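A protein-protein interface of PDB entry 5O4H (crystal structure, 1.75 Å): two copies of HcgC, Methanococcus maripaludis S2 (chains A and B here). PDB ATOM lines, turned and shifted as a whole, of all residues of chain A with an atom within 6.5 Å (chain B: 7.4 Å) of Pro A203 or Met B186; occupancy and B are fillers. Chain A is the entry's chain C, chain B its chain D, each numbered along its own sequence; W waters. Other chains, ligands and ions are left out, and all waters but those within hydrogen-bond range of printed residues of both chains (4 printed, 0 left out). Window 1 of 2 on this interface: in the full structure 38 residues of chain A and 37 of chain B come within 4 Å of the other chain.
O of Leu A205 lies close to O of Pro B203.
The backbone carbonyl oxygen (O) of Leu B205 sits close to the backbone carbonyl oxygen (O) of Pro A203.
The backbone carbonyl oxygen of Leu B205 lies within hydrogen-bond range of the backbone NH of Leu A205.
Of the 14 printed residues of chain A, 9 touch a printed residue of chain B.
Printed residues of chain A that touch a printed residue of chain B: Met A186, Cys A189, Thr A201, Ile A202, Pro A203, Asn A204, Leu A205, Lys A206 and Thr A231.
Hydrophobic or aromatic side chains of chain A within 4 Å of the printed part of chain B: Met A186, Ile A202, Pro A203 and Leu A205.
Hydrophobic or aromatic side chains of chain B within 4 Å of the printed part of chain A: Val B182, Met B186, Pro B203, Leu B205 and Tyr B207.
Among the printed residues, 17 pairs touch across the chains.
Met B186 touches its own counterpart, Met A186.
Met A186 touches Cys B189, and with the chains exchanged Cys A189 touches Met B186.
Asn A204 touches Lys B206, and with the chains exchanged Lys A206 touches Asn B204.
Leu B205 touches its own counterpart, Leu A205.
Positions printed for both chains: 185, 186, 189, 190, 201, 203, 204, 205, 206 and 230.
Water W2 lies within hydrogen-bond range of the side-chain carboxylate of Asp B183 (2.7 Å) and the backbone NH of Thr A201 (3.1 Å).
Water W1 lies within hydrogen-bond range of the side-chain amide oxygen (OD1) of Asn A204 (2.8 Å) and the backbone NH (N) of Tyr B207 (2.9 Å).
Water W3 lies within hydrogen-bond range of the backbone carbonyl oxygen (O) of Leu B205 and the backbone carbonyl oxygen (O) of Leu A205.
Water W4 lies within hydrogen-bond range of the guanidinium group (NH2) of Arg A190 and the guanidinium group (NE) of Arg B190.
The backbone NH of Ile A202 is in hydrogen-bond range of the backbone carbonyl oxygen of Thr A231 (2.8 Å).
The backbone carbonyl oxygen (O) of Ala A229 is in hydrogen-bond range of the backbone NH (N) of Asn A204 (3.0 Å).
The backbone carbonyl oxygen of Ile B185 lies within hydrogen-bond range of the side-chain sulfur of Cys B189.
The side-chain sulfur (SG) of Cys A189 sits at hydrogen-bond distance from the backbone carbonyl oxygen (O) of Ile A185, 3.3 Å away.
ND2 of Asn A204 sits at hydrogen-bond distance from O of Ser A228 (2.8 Å).
OG1 of Thr A231 lies within hydrogen-bond range of ND2 of Asn A204 (3.4 Å).
Pro A203 touches two residues of chain B.
Of the printed residues of chain A, Lys B206 touches Ile A202 and Asn A204.
Of the printed residues of chain A, Tyr B207 touches Asn A204 and Thr A231.
Of the printed residues of chain B, Ile A202 touches Val B182 (3.8 Å) and Lys B206 (3.3 Å).
The nearest residue of chain B that does not touch Pro A203 is Pro B203 (4.1 Å).
Among the printed residues, pairs that only touch across the chains: Ile A202 with Lys B206 (3.3 Å), Met A186 with Met B186 (3.7 Å), Lys A206 with Asn B204 (3.7 Å), Asn A204 with Lys B206 (3.7 Å), Thr A201 with Val B182 (3.7 Å), Cys A189 with Met B186 (3.7 Å), Met A186 with Cys B189 (3.7 Å), Pro A203 with Met B186 (3.7 Å), Ile A202 with Val B182 (3.8 Å), Asn A204 with Leu B205 (3.8 Å), Thr A231 with Tyr B207 (3.8 Å), Leu A205 with Asn B204 (3.8 Å), Met A186 with Pro B203 (3.8 Å) and Asn A204 with Tyr B207 (3.9 Å).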
ATOM      1  N   ILE A 185     -14.058  14.594 -31.532  1.00  0.00           N
ATOM      2  CA  ILE A 185     -13.745  14.962 -30.155  1.00  0.00           C
ATOM      3  C   ILE A 185     -12.904  16.238 -30.105  1.00  0.00           C
ATOM      4  O   ILE A 185     -13.192  17.117 -29.296  1.00  0.00           O
ATOM      5  CB  ILE A 185     -13.076  13.764 -29.429  1.00  0.00           C
ATOM      6  CG1 ILE A 185     -14.104  12.633 -29.260  1.00  0.00           C
ATOM      7  CG2 ILE A 185     -12.456  14.180 -28.101  1.00  0.00           C
ATOM      8  CD1 ILE A 185     -13.485  11.278 -28.712  1.00  0.00           C
ATOM      9  N   MET A 186     -11.900  16.333 -30.947  1.00  0.00           N
ATOM     10  CA  MET A 186     -11.018  17.502 -30.999  1.00  0.00           C
ATOM     11  C   MET A 186     -11.801  18.760 -31.374  1.00  0.00           C
ATOM     12  O   MET A 186     -11.650  19.775 -30.701  1.00  0.00           O
ATOM     13  CB  MET A 186      -9.846  17.291 -31.967  1.00  0.00           C
ATOM     14  CG  MET A 186      -8.866  16.238 -31.482  1.00  0.00           C
ATOM     15  SD  MET A 186      -8.007  16.619 -29.938  1.00  0.00           S
ATOM     16  CE  MET A 186      -6.838  17.882 -30.551  1.00  0.00           C
ATOM     17  N   CYS A 189     -14.025  19.776 -28.448  1.00  0.00           N
ATOM     18  CA  CYS A 189     -13.237  20.429 -27.383  1.00  0.00           C
ATOM     19  C   CYS A 189     -12.995  21.888 -27.701  1.00  0.00           C
ATOM     20  O   CYS A 189     -13.128  22.732 -26.830  1.00  0.00           O
ATOM     21  CB  CYS A 189     -11.911  19.713 -27.170  1.00  0.00           C
ATOM     22  SG  CYS A 189     -12.082  18.149 -26.322  1.00  0.00           S
ATOM     23  N   ARG A 190     -12.641  22.176 -28.949  1.00  0.00           N
ATOM     24  CA  ARG A 190     -12.382  23.550 -29.389  1.00  0.00           C
ATOM     25  C   ARG A 190     -13.575  24.477 -29.102  1.00  0.00           C
ATOM     26  O   ARG A 190     -13.426  25.581 -28.549  1.00  0.00           O
ATOM     27  CB  ARG A 190     -12.007  23.574 -30.907  1.00  0.00           C
ATOM     28  CG  ARG A 190     -11.794  24.960 -31.541  1.00  0.00           C
ATOM     29  CD  ARG A 190     -11.410  24.852 -33.007  1.00  0.00           C
ATOM     30  NE  ARG A 190     -11.655  26.106 -33.731  1.00  0.00           N
ATOM     31  CZ  ARG A 190     -11.092  26.460 -34.889  1.00  0.00           C
ATOM     32  NH1 ARG A 190     -11.397  27.627 -35.452  1.00  0.00           N
ATOM     33  NH2 ARG A 190     -10.215  25.655 -35.491  1.00  0.00           N
ATOM     34  N   THR A 201     -10.796  22.098 -21.118  1.00  0.00           N
ATOM     35  CA  THR A 201     -11.510  20.997 -21.737  1.00  0.00           C
ATOM     36  C   THR A 201     -10.525  19.940 -22.111  1.00  0.00           C
ATOM     37  O   THR A 201      -9.573  20.209 -22.846  1.00  0.00           O
ATOM     38  CB  THR A 201     -12.233  21.516 -22.978  1.00  0.00           C
ATOM     39  OG1 THR A 201     -12.990  22.690 -22.660  1.00  0.00           O
ATOM     40  CG2 THR A 201     -13.171  20.504 -23.538  1.00  0.00           C
ATOM     41  N   ILE A 202     -10.762  18.726 -21.649  1.00  0.00           N
ATOM     42  CA  ILE A 202      -9.862  17.626 -21.943  1.00  0.00           C
ATOM     43  C   ILE A 202     -10.476  16.507 -22.760  1.00  0.00           C
ATOM     44  O   ILE A 202     -11.455  15.919 -22.337  1.00  0.00           O
ATOM     45  CB  ILE A 202      -9.248  17.068 -20.612  1.00  0.00           C
ATOM     46  CG1 ILE A 202      -8.167  18.069 -20.103  1.00  0.00           C
ATOM     47  CG2 ILE A 202      -8.594  15.680 -20.862  1.00  0.00           C
ATOM     48  CD1 ILE A 202      -7.342  17.695 -18.910  1.00  0.00           C
ATOM     49  N   PRO A 203      -9.878  16.166 -23.916  1.00  0.00           N
ATOM     50  CA  PRO A 203     -10.380  15.036 -24.704  1.00  0.00           C
ATOM     51  C   PRO A 203      -9.716  13.800 -24.067  1.00  0.00           C
ATOM     52  O   PRO A 203      -8.531  13.848 -23.766  1.00  0.00           O
ATOM     53  CB  PRO A 203      -9.815  15.317 -26.099  1.00  0.00           C
ATOM     54  CG  PRO A 203      -8.552  16.042 -25.843  1.00  0.00           C
ATOM     55  CD  PRO A 203      -8.681  16.771 -24.553  1.00  0.00           C
ATOM     56  N   ASN A 204     -10.449  12.706 -23.843  1.00  0.00           N
ATOM     57  CA  ASN A 204      -9.870  11.508 -23.234  1.00  0.00           C
ATOM     58  C   ASN A 204      -9.374  10.714 -24.390  1.00  0.00           C
ATOM     59  O   ASN A 204     -10.074   9.863 -24.914  1.00  0.00           O
ATOM     60  CB  ASN A 204     -10.914  10.740 -22.449  1.00  0.00           C
ATOM     61  CG  ASN A 204     -11.184  11.440 -21.155  1.00  0.00           C
ATOM     62  OD1 ASN A 204     -10.252  11.759 -20.419  1.00  0.00           O
ATOM     63  ND2 ASN A 204     -12.417  11.838 -20.911  1.00  0.00           N
ATOM     64  N   LEU A 205      -8.155  11.002 -24.807  1.00  0.00           N
ATOM     65  CA  LEU A 205      -7.582  10.325 -25.957  1.00  0.00           C
ATOM     66  C   LEU A 205      -6.238   9.746 -25.669  1.00  0.00           C
ATOM     67  O   LEU A 205      -5.510  10.204 -24.789  1.00  0.00           O
ATOM     68  CB  LEU A 205      -7.466  11.330 -27.119  1.00  0.00           C
ATOM     69  CG  LEU A 205      -8.778  11.871 -27.677  1.00  0.00           C
ATOM     70  CD1 LEU A 205      -8.529  13.026 -28.621  1.00  0.00           C
ATOM     71  CD2 LEU A 205      -9.565  10.807 -28.399  1.00  0.00           C
ATOM     72  N   LYS A 206      -5.901   8.718 -26.443  1.00  0.00           N
ATOM     73  CA  LYS A 206      -4.621   8.033 -26.347  1.00  0.00           C
ATOM     74  C   LYS A 206      -4.377   7.330 -27.653  1.00  0.00           C
ATOM     75  O   LYS A 206      -5.252   7.320 -28.529  1.00  0.00           O
ATOM     76  CB  LYS A 206      -4.580   7.073 -25.159  1.00  0.00           C
ATOM     77  CG  LYS A 206      -5.573   5.920 -25.226  1.00  0.00           C
ATOM     78  CD  LYS A 206      -5.278   4.897 -24.156  1.00  0.00           C
ATOM     79  CE  LYS A 206      -4.174   3.947 -24.573  1.00  0.00           C
ATOM     80  NZ  LYS A 206      -3.618   3.201 -23.410  1.00  0.00           N
ATOM     81  N   SER A 228     -15.809   8.457 -20.979  1.00  0.00           N
ATOM     82  CA  SER A 228     -16.283   9.741 -21.477  1.00  0.00           C
ATOM     83  C   SER A 228     -15.382  10.283 -22.510  1.00  0.00           C
ATOM     84  O   SER A 228     -14.149  10.219 -22.359  1.00  0.00           O
ATOM     85  CB  SER A 228     -16.389  10.777 -20.352  1.00  0.00           C
ATOM     86  OG  SER A 228     -17.399  10.344 -19.466  1.00  0.00           O
ATOM     87  N   ALA A 229     -15.975  10.827 -23.564  1.00  0.00           N
ATOM     88  CA  ALA A 229     -15.181  11.423 -24.626  1.00  0.00           C
ATOM     89  C   ALA A 229     -14.458  12.689 -24.154  1.00  0.00           C
ATOM     90  O   ALA A 229     -13.312  12.924 -24.538  1.00  0.00           O
ATOM     91  CB  ALA A 229     -16.077  11.764 -25.797  1.00  0.00           C
ATOM     92  N   ILE A 230     -15.112  13.504 -23.320  1.00  0.00           N
ATOM     93  CA  ILE A 230     -14.551  14.765 -22.836  1.00  0.00           C
ATOM     94  C   ILE A 230     -14.868  15.038 -21.389  1.00  0.00           C
ATOM     95  O   ILE A 230     -15.956  14.697 -20.915  1.00  0.00           O
ATOM     96  CB  ILE A 230     -15.207  15.916 -23.690  1.00  0.00           C
ATOM     97  CG1 ILE A 230     -14.788  15.812 -25.171  1.00  0.00           C
ATOM     98  CG2 ILE A 230     -14.850  17.349 -23.146  1.00  0.00           C
ATOM     99  CD1 ILE A 230     -15.500  16.751 -26.115  1.00  0.00           C
ATOM    100  N   THR A 231     -13.911  15.691 -20.714  1.00  0.00           N
ATOM    101  CA  THR A 231     -14.033  16.130 -19.333  1.00  0.00           C
ATOM    102  C   THR A 231     -13.846  17.643 -19.385  1.00  0.00           C
ATOM    103  O   THR A 231     -12.901  18.145 -19.998  1.00  0.00           O
ATOM    104  CB  THR A 231     -13.047  15.455 -18.373  1.00  0.00           C
ATOM    105  OG1 THR A 231     -13.203  14.041 -18.496  1.00  0.00           O
ATOM    106  CG2 THR A 231     -13.303  15.845 -16.951  1.00  0.00           C
ATOM    107  N   ARG B 167      -0.128  32.897 -22.676  1.00  0.00           N
ATOM    108  CA  ARG B 167       0.506  32.325 -23.864  1.00  0.00           C
ATOM    109  C   ARG B 167       0.454  33.476 -24.857  1.00  0.00           C
ATOM    110  O   ARG B 167      -0.613  33.933 -25.267  1.00  0.00           O
ATOM    111  CB  ARG B 167      -0.214  31.093 -24.396  1.00  0.00           C
ATOM    112  CG  ARG B 167      -0.239  29.991 -23.374  1.00  0.00           C
ATOM    113  CD  ARG B 167      -0.631  28.666 -23.986  1.00  0.00           C
ATOM    114  NE  ARG B 167      -1.978  28.733 -24.552  1.00  0.00           N
ATOM    115  CZ  ARG B 167      -2.373  28.325 -25.754  1.00  0.00           C
ATOM    116  NH1 ARG B 167      -3.630  28.442 -26.128  1.00  0.00           N
ATOM    117  NH2 ARG B 167      -1.502  27.797 -26.597  1.00  0.00           N
ATOM    118  N   THR B 179      -3.908  23.933 -17.224  1.00  0.00           N
ATOM    119  CA  THR B 179      -4.675  24.518 -18.331  1.00  0.00           C
ATOM    120  C   THR B 179      -3.724  24.928 -19.439  1.00  0.00           C
ATOM    121  O   THR B 179      -4.011  24.683 -20.606  1.00  0.00           O
ATOM    122  CB  THR B 179      -5.417  25.805 -17.890  1.00  0.00           C
ATOM    123  OG1 THR B 179      -6.403  25.466 -16.933  1.00  0.00           O
ATOM    124  CG2 THR B 179      -6.101  26.538 -19.053  1.00  0.00           C
ATOM    125  N   LEU B 180      -2.615  25.579 -19.052  1.00  0.00           N
ATOM    126  CA  LEU B 180      -1.631  26.034 -20.034  1.00  0.00           C
ATOM    127  C   LEU B 180      -1.024  24.847 -20.768  1.00  0.00           C
ATOM    128  O   LEU B 180      -0.836  24.908 -21.981  1.00  0.00           O
ATOM    129  CB  LEU B 180      -0.549  26.882 -19.384  1.00  0.00           C
ATOM    130  CG  LEU B 180      -0.972  28.233 -18.857  1.00  0.00           C
ATOM    131  CD1 LEU B 180       0.097  28.856 -18.054  1.00  0.00           C
ATOM    132  CD2 LEU B 180      -1.352  29.192 -19.967  1.00  0.00           C
ATOM    133  N   VAL B 181      -0.733  23.769 -20.062  1.00  0.00           N
ATOM    134  CA  VAL B 181      -0.146  22.563 -20.679  1.00  0.00           C
ATOM    135  C   VAL B 181      -1.153  21.954 -21.648  1.00  0.00           C
ATOM    136  O   VAL B 181      -0.808  21.613 -22.768  1.00  0.00           O
ATOM    137  CB  VAL B 181       0.285  21.565 -19.580  1.00  0.00           C
ATOM    138  CG1 VAL B 181       0.643  20.195 -20.155  1.00  0.00           C
ATOM    139  CG2 VAL B 181       1.471  22.124 -18.811  1.00  0.00           C
ATOM    140  N   VAL B 182      -2.398  21.817 -21.218  1.00  0.00           N
ATOM    141  CA  VAL B 182      -3.440  21.254 -22.076  1.00  0.00           C
ATOM    142  C   VAL B 182      -3.591  22.097 -23.338  1.00  0.00           C
ATOM    143  O   VAL B 182      -3.648  21.555 -24.438  1.00  0.00           O
ATOM    144  CB  VAL B 182      -4.783  21.139 -21.297  1.00  0.00           C
ATOM    145  CG1 VAL B 182      -5.963  20.910 -22.235  1.00  0.00           C
ATOM    146  CG2 VAL B 182      -4.702  20.009 -20.279  1.00  0.00           C
ATOM    147  N   ASP B 183      -3.647  23.418 -23.179  1.00  0.00           N
ATOM    148  CA  ASP B 183      -3.799  24.356 -24.304  1.00  0.00           C
ATOM    149  C   ASP B 183      -2.623  24.288 -25.266  1.00  0.00           C
ATOM    150  O   ASP B 183      -2.858  24.319 -26.464  1.00  0.00           O
ATOM    151  CB  ASP B 183      -4.064  25.759 -23.792  1.00  0.00           C
ATOM    152  CG  ASP B 183      -5.452  25.892 -23.161  1.00  0.00           C
ATOM    153  OD1 ASP B 183      -6.310  24.964 -23.362  1.00  0.00           O
ATOM    154  OD2 ASP B 183      -5.697  26.912 -22.510  1.00  0.00           O
ATOM    155  N   ILE B 184      -1.393  24.159 -24.765  1.00  0.00           N
ATOM    156  CA  ILE B 184      -0.205  24.034 -25.616  1.00  0.00           C
ATOM    157  C   ILE B 184      -0.335  22.763 -26.462  1.00  0.00           C
ATOM    158  O   ILE B 184      -0.062  22.782 -27.662  1.00  0.00           O
ATOM    159  CB  ILE B 184       1.058  23.948 -24.722  1.00  0.00           C
ATOM    160  CG1 ILE B 184       1.446  25.327 -24.210  1.00  0.00           C
ATOM    161  CG2 ILE B 184       2.252  23.290 -25.457  1.00  0.00           C
ATOM    162  CD1 ILE B 184       2.329  25.317 -23.041  1.00  0.00           C
ATOM    163  N   ILE B 185      -0.728  21.677 -25.836  1.00  0.00           N
ATOM    164  CA  ILE B 185      -0.866  20.395 -26.535  1.00  0.00           C
ATOM    165  C   ILE B 185      -1.976  20.442 -27.557  1.00  0.00           C
ATOM    166  O   ILE B 185      -1.800  19.984 -28.670  1.00  0.00           O
ATOM    167  CB  ILE B 185      -1.015  19.241 -25.513  1.00  0.00           C
ATOM    168  CG1 ILE B 185       0.283  19.064 -24.726  1.00  0.00           C
ATOM    169  CG2 ILE B 185      -1.456  17.933 -26.197  1.00  0.00           C
ATOM    170  CD1 ILE B 185       0.184  18.046 -23.527  1.00  0.00           C
ATOM    171  N   MET B 186      -3.128  20.994 -27.181  1.00  0.00           N
ATOM    172  CA  MET B 186      -4.274  21.089 -28.076  1.00  0.00           C
ATOM    173  C   MET B 186      -3.936  21.941 -29.287  1.00  0.00           C
ATOM    174  O   MET B 186      -4.194  21.507 -30.402  1.00  0.00           O
ATOM    175  CB  MET B 186      -5.502  21.637 -27.347  1.00  0.00           C
ATOM    176  CG  MET B 186      -6.049  20.679 -26.310  1.00  0.00           C
ATOM    177  SD  MET B 186      -6.693  19.095 -26.952  1.00  0.00           S
ATOM    178  CE  MET B 186      -8.215  19.655 -27.672  1.00  0.00           C
ATOM    179  N   ASP B 187      -3.356  23.142 -29.080  1.00  0.00           N
ATOM    180  CA  ASP B 187      -2.986  24.013 -30.188  1.00  0.00           C
ATOM    181  C   ASP B 187      -1.952  23.365 -31.061  1.00  0.00           C
ATOM    182  O   ASP B 187      -2.007  23.540 -32.278  1.00  0.00           O
ATOM    183  CB  ASP B 187      -2.475  25.379 -29.703  1.00  0.00           C
ATOM    184  CG  ASP B 187      -3.562  26.351 -29.284  1.00  0.00           C
ATOM    185  OD1 ASP B 187      -4.746  26.065 -29.531  1.00  0.00           O
ATOM    186  OD2 ASP B 187      -3.229  27.400 -28.701  1.00  0.00           O
ATOM    187  N   SER B 188      -1.007  22.630 -30.457  1.00  0.00           N
ATOM    188  CA  SER B 188       0.034  21.944 -31.210  1.00  0.00           C
ATOM    189  C   SER B 188      -0.595  20.877 -32.102  1.00  0.00           C
ATOM    190  O   SER B 188      -0.245  20.789 -33.277  1.00  0.00           O
ATOM    191  CB  SER B 188       1.079  21.356 -30.267  1.00  0.00           C
ATOM    192  OG  SER B 188       1.784  22.399 -29.621  1.00  0.00           O
ATOM    193  N   CYS B 189      -1.545  20.075 -31.574  1.00  0.00           N
ATOM    194  CA  CYS B 189      -2.234  19.040 -32.368  1.00  0.00           C
ATOM    195  C   CYS B 189      -2.915  19.615 -33.580  1.00  0.00           C
ATOM    196  O   CYS B 189      -2.816  19.052 -34.671  1.00  0.00           O
ATOM    197  CB  CYS B 189      -3.253  18.298 -31.516  1.00  0.00           C
ATOM    198  SG  CYS B 189      -2.500  17.168 -30.350  1.00  0.00           S
ATOM    199  N   ARG B 190      -3.622  20.717 -33.400  1.00  0.00           N
ATOM    200  CA  ARG B 190      -4.327  21.343 -34.511  1.00  0.00           C
ATOM    201  C   ARG B 190      -3.363  21.711 -35.634  1.00  0.00           C
ATOM    202  O   ARG B 190      -3.651  21.434 -36.785  1.00  0.00           O
ATOM    203  CB  ARG B 190      -5.167  22.555 -34.035  1.00  0.00           C
ATOM    204  CG  ARG B 190      -6.410  22.138 -33.249  1.00  0.00           C
ATOM    205  CD  ARG B 190      -7.329  23.314 -32.925  1.00  0.00           C
ATOM    206  NE  ARG B 190      -6.918  24.039 -31.717  1.00  0.00           N
ATOM    207  CZ  ARG B 190      -7.272  23.732 -30.469  1.00  0.00           C
ATOM    208  NH1 ARG B 190      -6.838  24.462 -29.453  1.00  0.00           N
ATOM    209  NH2 ARG B 190      -8.062  22.693 -30.228  1.00  0.00           N
ATOM    210  N   GLU B 191      -2.217  22.294 -35.310  1.00  0.00           N
ATOM    211  CA  GLU B 191      -1.245  22.671 -36.322  1.00  0.00           C
ATOM    212  C   GLU B 191      -0.544  21.461 -36.930  1.00  0.00           C
ATOM    213  O   GLU B 191      -0.278  21.428 -38.131  1.00  0.00           O
ATOM    214  CB  GLU B 191      -0.256  23.651 -35.723  1.00  0.00           C
ATOM    215  CG  GLU B 191       0.682  24.247 -36.733  1.00  0.00           C
ATOM    216  CD  GLU B 191       1.611  25.314 -36.198  1.00  0.00           C
ATOM    217  OE1 GLU B 191       1.437  25.748 -35.038  1.00  0.00           O
ATOM    218  OE2 GLU B 191       2.562  25.669 -36.922  1.00  0.00           O
ATOM    219  N   ILE B 192      -0.227  20.460 -36.101  1.00  0.00           N
ATOM    220  CA  ILE B 192       0.446  19.257 -36.589  1.00  0.00           C
ATOM    221  C   ILE B 192      -0.454  18.535 -37.584  1.00  0.00           C
ATOM    222  O   ILE B 192       0.036  18.015 -38.591  1.00  0.00           O
ATOM    223  CB  ILE B 192       0.840  18.337 -35.408  1.00  0.00           C
ATOM    224  CG1 ILE B 192       2.006  18.950 -34.623  1.00  0.00           C
ATOM    225  CG2 ILE B 192       1.220  16.928 -35.888  1.00  0.00           C
ATOM    226  CD1 ILE B 192       2.097  18.476 -33.185  1.00  0.00           C
ATOM    227  N   THR B 201      -3.535  12.929 -35.532  1.00  0.00           N
ATOM    228  CA  THR B 201      -2.749  13.442 -34.425  1.00  0.00           C
ATOM    229  C   THR B 201      -3.511  13.222 -33.157  1.00  0.00           C
ATOM    230  O   THR B 201      -4.642  13.678 -33.043  1.00  0.00           O
ATOM    231  CB  THR B 201      -2.490  14.944 -34.634  1.00  0.00           C
ATOM    232  OG1 THR B 201      -2.011  15.183 -35.961  1.00  0.00           O
ATOM    233  CG2 THR B 201      -1.489  15.472 -33.673  1.00  0.00           C
ATOM    234  N   PRO B 203      -3.592  13.696 -28.974  1.00  0.00           N
ATOM    235  CA  PRO B 203      -2.950  14.223 -27.766  1.00  0.00           C
ATOM    236  C   PRO B 203      -3.091  13.161 -26.684  1.00  0.00           C
ATOM    237  O   PRO B 203      -4.105  12.459 -26.630  1.00  0.00           O
ATOM    238  CB  PRO B 203      -3.810  15.444 -27.414  1.00  0.00           C
ATOM    239  CG  PRO B 203      -5.151  15.102 -27.889  1.00  0.00           C
ATOM    240  CD  PRO B 203      -4.975  14.210 -29.108  1.00  0.00           C
ATOM    241  N   ASN B 204      -2.084  13.020 -25.827  1.00  0.00           N
ATOM    242  CA  ASN B 204      -2.179  12.025 -24.770  1.00  0.00           C
ATOM    243  C   ASN B 204      -2.672  12.766 -23.571  1.00  0.00           C
ATOM    244  O   ASN B 204      -1.883  13.210 -22.776  1.00  0.00           O
ATOM    245  CB  ASN B 204      -0.832  11.378 -24.516  1.00  0.00           C
ATOM    246  CG  ASN B 204      -0.501  10.409 -25.622  1.00  0.00           C
ATOM    247  OD1 ASN B 204      -1.310   9.543 -25.932  1.00  0.00           O
ATOM    248  ND2 ASN B 204       0.607  10.608 -26.319  1.00  0.00           N
ATOM    249  N   LEU B 205      -3.986  12.914 -23.459  1.00  0.00           N
ATOM    250  CA  LEU B 205      -4.567  13.650 -22.352  1.00  0.00           C
ATOM    251  C   LEU B 205      -5.623  12.880 -21.637  1.00  0.00           C
ATOM    252  O   LEU B 205      -6.275  11.994 -22.193  1.00  0.00           O
ATOM    253  CB  LEU B 205      -5.162  14.983 -22.867  1.00  0.00           C
ATOM    254  CG  LEU B 205      -4.198  15.990 -23.447  1.00  0.00           C
ATOM    255  CD1 LEU B 205      -4.930  17.105 -24.159  1.00  0.00           C
ATOM    256  CD2 LEU B 205      -3.317  16.604 -22.387  1.00  0.00           C
ATOM    257  N   LYS B 206      -5.795  13.228 -20.371  1.00  0.00           N
ATOM    258  CA  LYS B 206      -6.797  12.631 -19.507  1.00  0.00           C
ATOM    259  C   LYS B 206      -7.068  13.617 -18.396  1.00  0.00           C
ATOM    260  O   LYS B 206      -6.363  14.639 -18.299  1.00  0.00           O
ATOM    261  CB  LYS B 206      -6.352  11.270 -18.962  1.00  0.00           C
ATOM    262  CG  LYS B 206      -5.118  11.305 -18.080  1.00  0.00           C
ATOM    263  CD  LYS B 206      -4.927   9.970 -17.377  1.00  0.00           C
ATOM    264  CE  LYS B 206      -5.797   9.843 -16.147  1.00  0.00           C
ATOM    265  NZ  LYS B 206      -5.907   8.434 -15.687  1.00  0.00           N
ATOM    266  N   TYR B 207      -8.052  13.336 -17.560  1.00  0.00           N
ATOM    267  CA  TYR B 207      -8.387  14.231 -16.462  1.00  0.00           C
ATOM    268  C   TYR B 207      -7.368  14.019 -15.327  1.00  0.00           C
ATOM    269  O   TYR B 207      -7.620  13.331 -14.351  1.00  0.00           O
ATOM    270  CB  TYR B 207      -9.827  14.008 -16.030  1.00  0.00           C
ATOM    271  CG  TYR B 207     -10.275  14.886 -14.880  1.00  0.00           C
ATOM    272  CD1 TYR B 207     -10.095  16.265 -14.920  1.00  0.00           C
ATOM    273  CD2 TYR B 207     -10.913  14.347 -13.778  1.00  0.00           C
ATOM    274  CE1 TYR B 207     -10.506  17.077 -13.861  1.00  0.00           C
ATOM    275  CE2 TYR B 207     -11.328  15.145 -12.721  1.00  0.00           C
ATOM    276  CZ  TYR B 207     -11.122  16.513 -12.764  1.00  0.00           C
ATOM    277  OH  TYR B 207     -11.542  17.300 -11.712  1.00  0.00           O
ATOM    278  N   ILE B 230       2.230  14.027 -27.631  1.00  0.00           N
ATOM    279  CA  ILE B 230       1.453  13.745 -28.838  1.00  0.00           C
ATOM    280  C   ILE B 230       1.990  12.556 -29.606  1.00  0.00           C
ATOM    281  O   ILE B 230       3.197  12.332 -29.627  1.00  0.00           O
ATOM    282  CB  ILE B 230       1.575  15.019 -29.749  1.00  0.00           C
ATOM    283  CG1 ILE B 230       0.905  16.245 -29.094  1.00  0.00           C
ATOM    284  CG2 ILE B 230       1.000  14.776 -31.175  1.00  0.00           C
ATOM    285  CD1 ILE B 230       1.130  17.555 -29.794  1.00  0.00           C
ATOM    286  N   LEU B 246       5.552  22.036 -31.123  1.00  0.00           N
ATOM    287  CA  LEU B 246       5.424  21.967 -29.667  1.00  0.00           C
ATOM    288  C   LEU B 246       6.324  22.960 -28.992  1.00  0.00           C
ATOM    289  O   LEU B 246       5.864  23.675 -28.137  1.00  0.00           O
ATOM    290  CB  LEU B 246       5.766  20.567 -29.107  1.00  0.00           C
ATOM    291  CG  LEU B 246       4.652  19.573 -29.095  1.00  0.00           C
ATOM    292  CD1 LEU B 246       5.184  18.183 -28.859  1.00  0.00           C
ATOM    293  CD2 LEU B 246       3.620  19.902 -27.990  1.00  0.00           C
ATOM    294  N   ASN B 249       5.066  26.476 -29.227  1.00  0.00           N
ATOM    295  CA  ASN B 249       3.934  26.713 -28.335  1.00  0.00           C
ATOM    296  C   ASN B 249       4.362  26.821 -26.890  1.00  0.00           C
ATOM    297  O   ASN B 249       3.809  27.607 -26.142  1.00  0.00           O
ATOM    298  CB  ASN B 249       2.835  25.669 -28.528  1.00  0.00           C
ATOM    299  CG  ASN B 249       1.910  26.055 -29.646  1.00  0.00           C
ATOM    300  OD1 ASN B 249       1.349  27.166 -29.652  1.00  0.00           O
ATOM    301  ND2 ASN B 249       1.762  25.207 -30.622  1.00  0.00           N
HETATM  302  O   HOH W   1      -9.878  11.131 -17.747  1.00  0.00           O
HETATM  303  O   HOH W   2      -8.622  23.709 -22.615  1.00  0.00           O
HETATM  304  O   HOH W   3      -7.089   9.338 -21.944  1.00  0.00           O
HETATM  305  O   HOH W   4      -8.464  26.337 -33.319  1.00  0.00           O
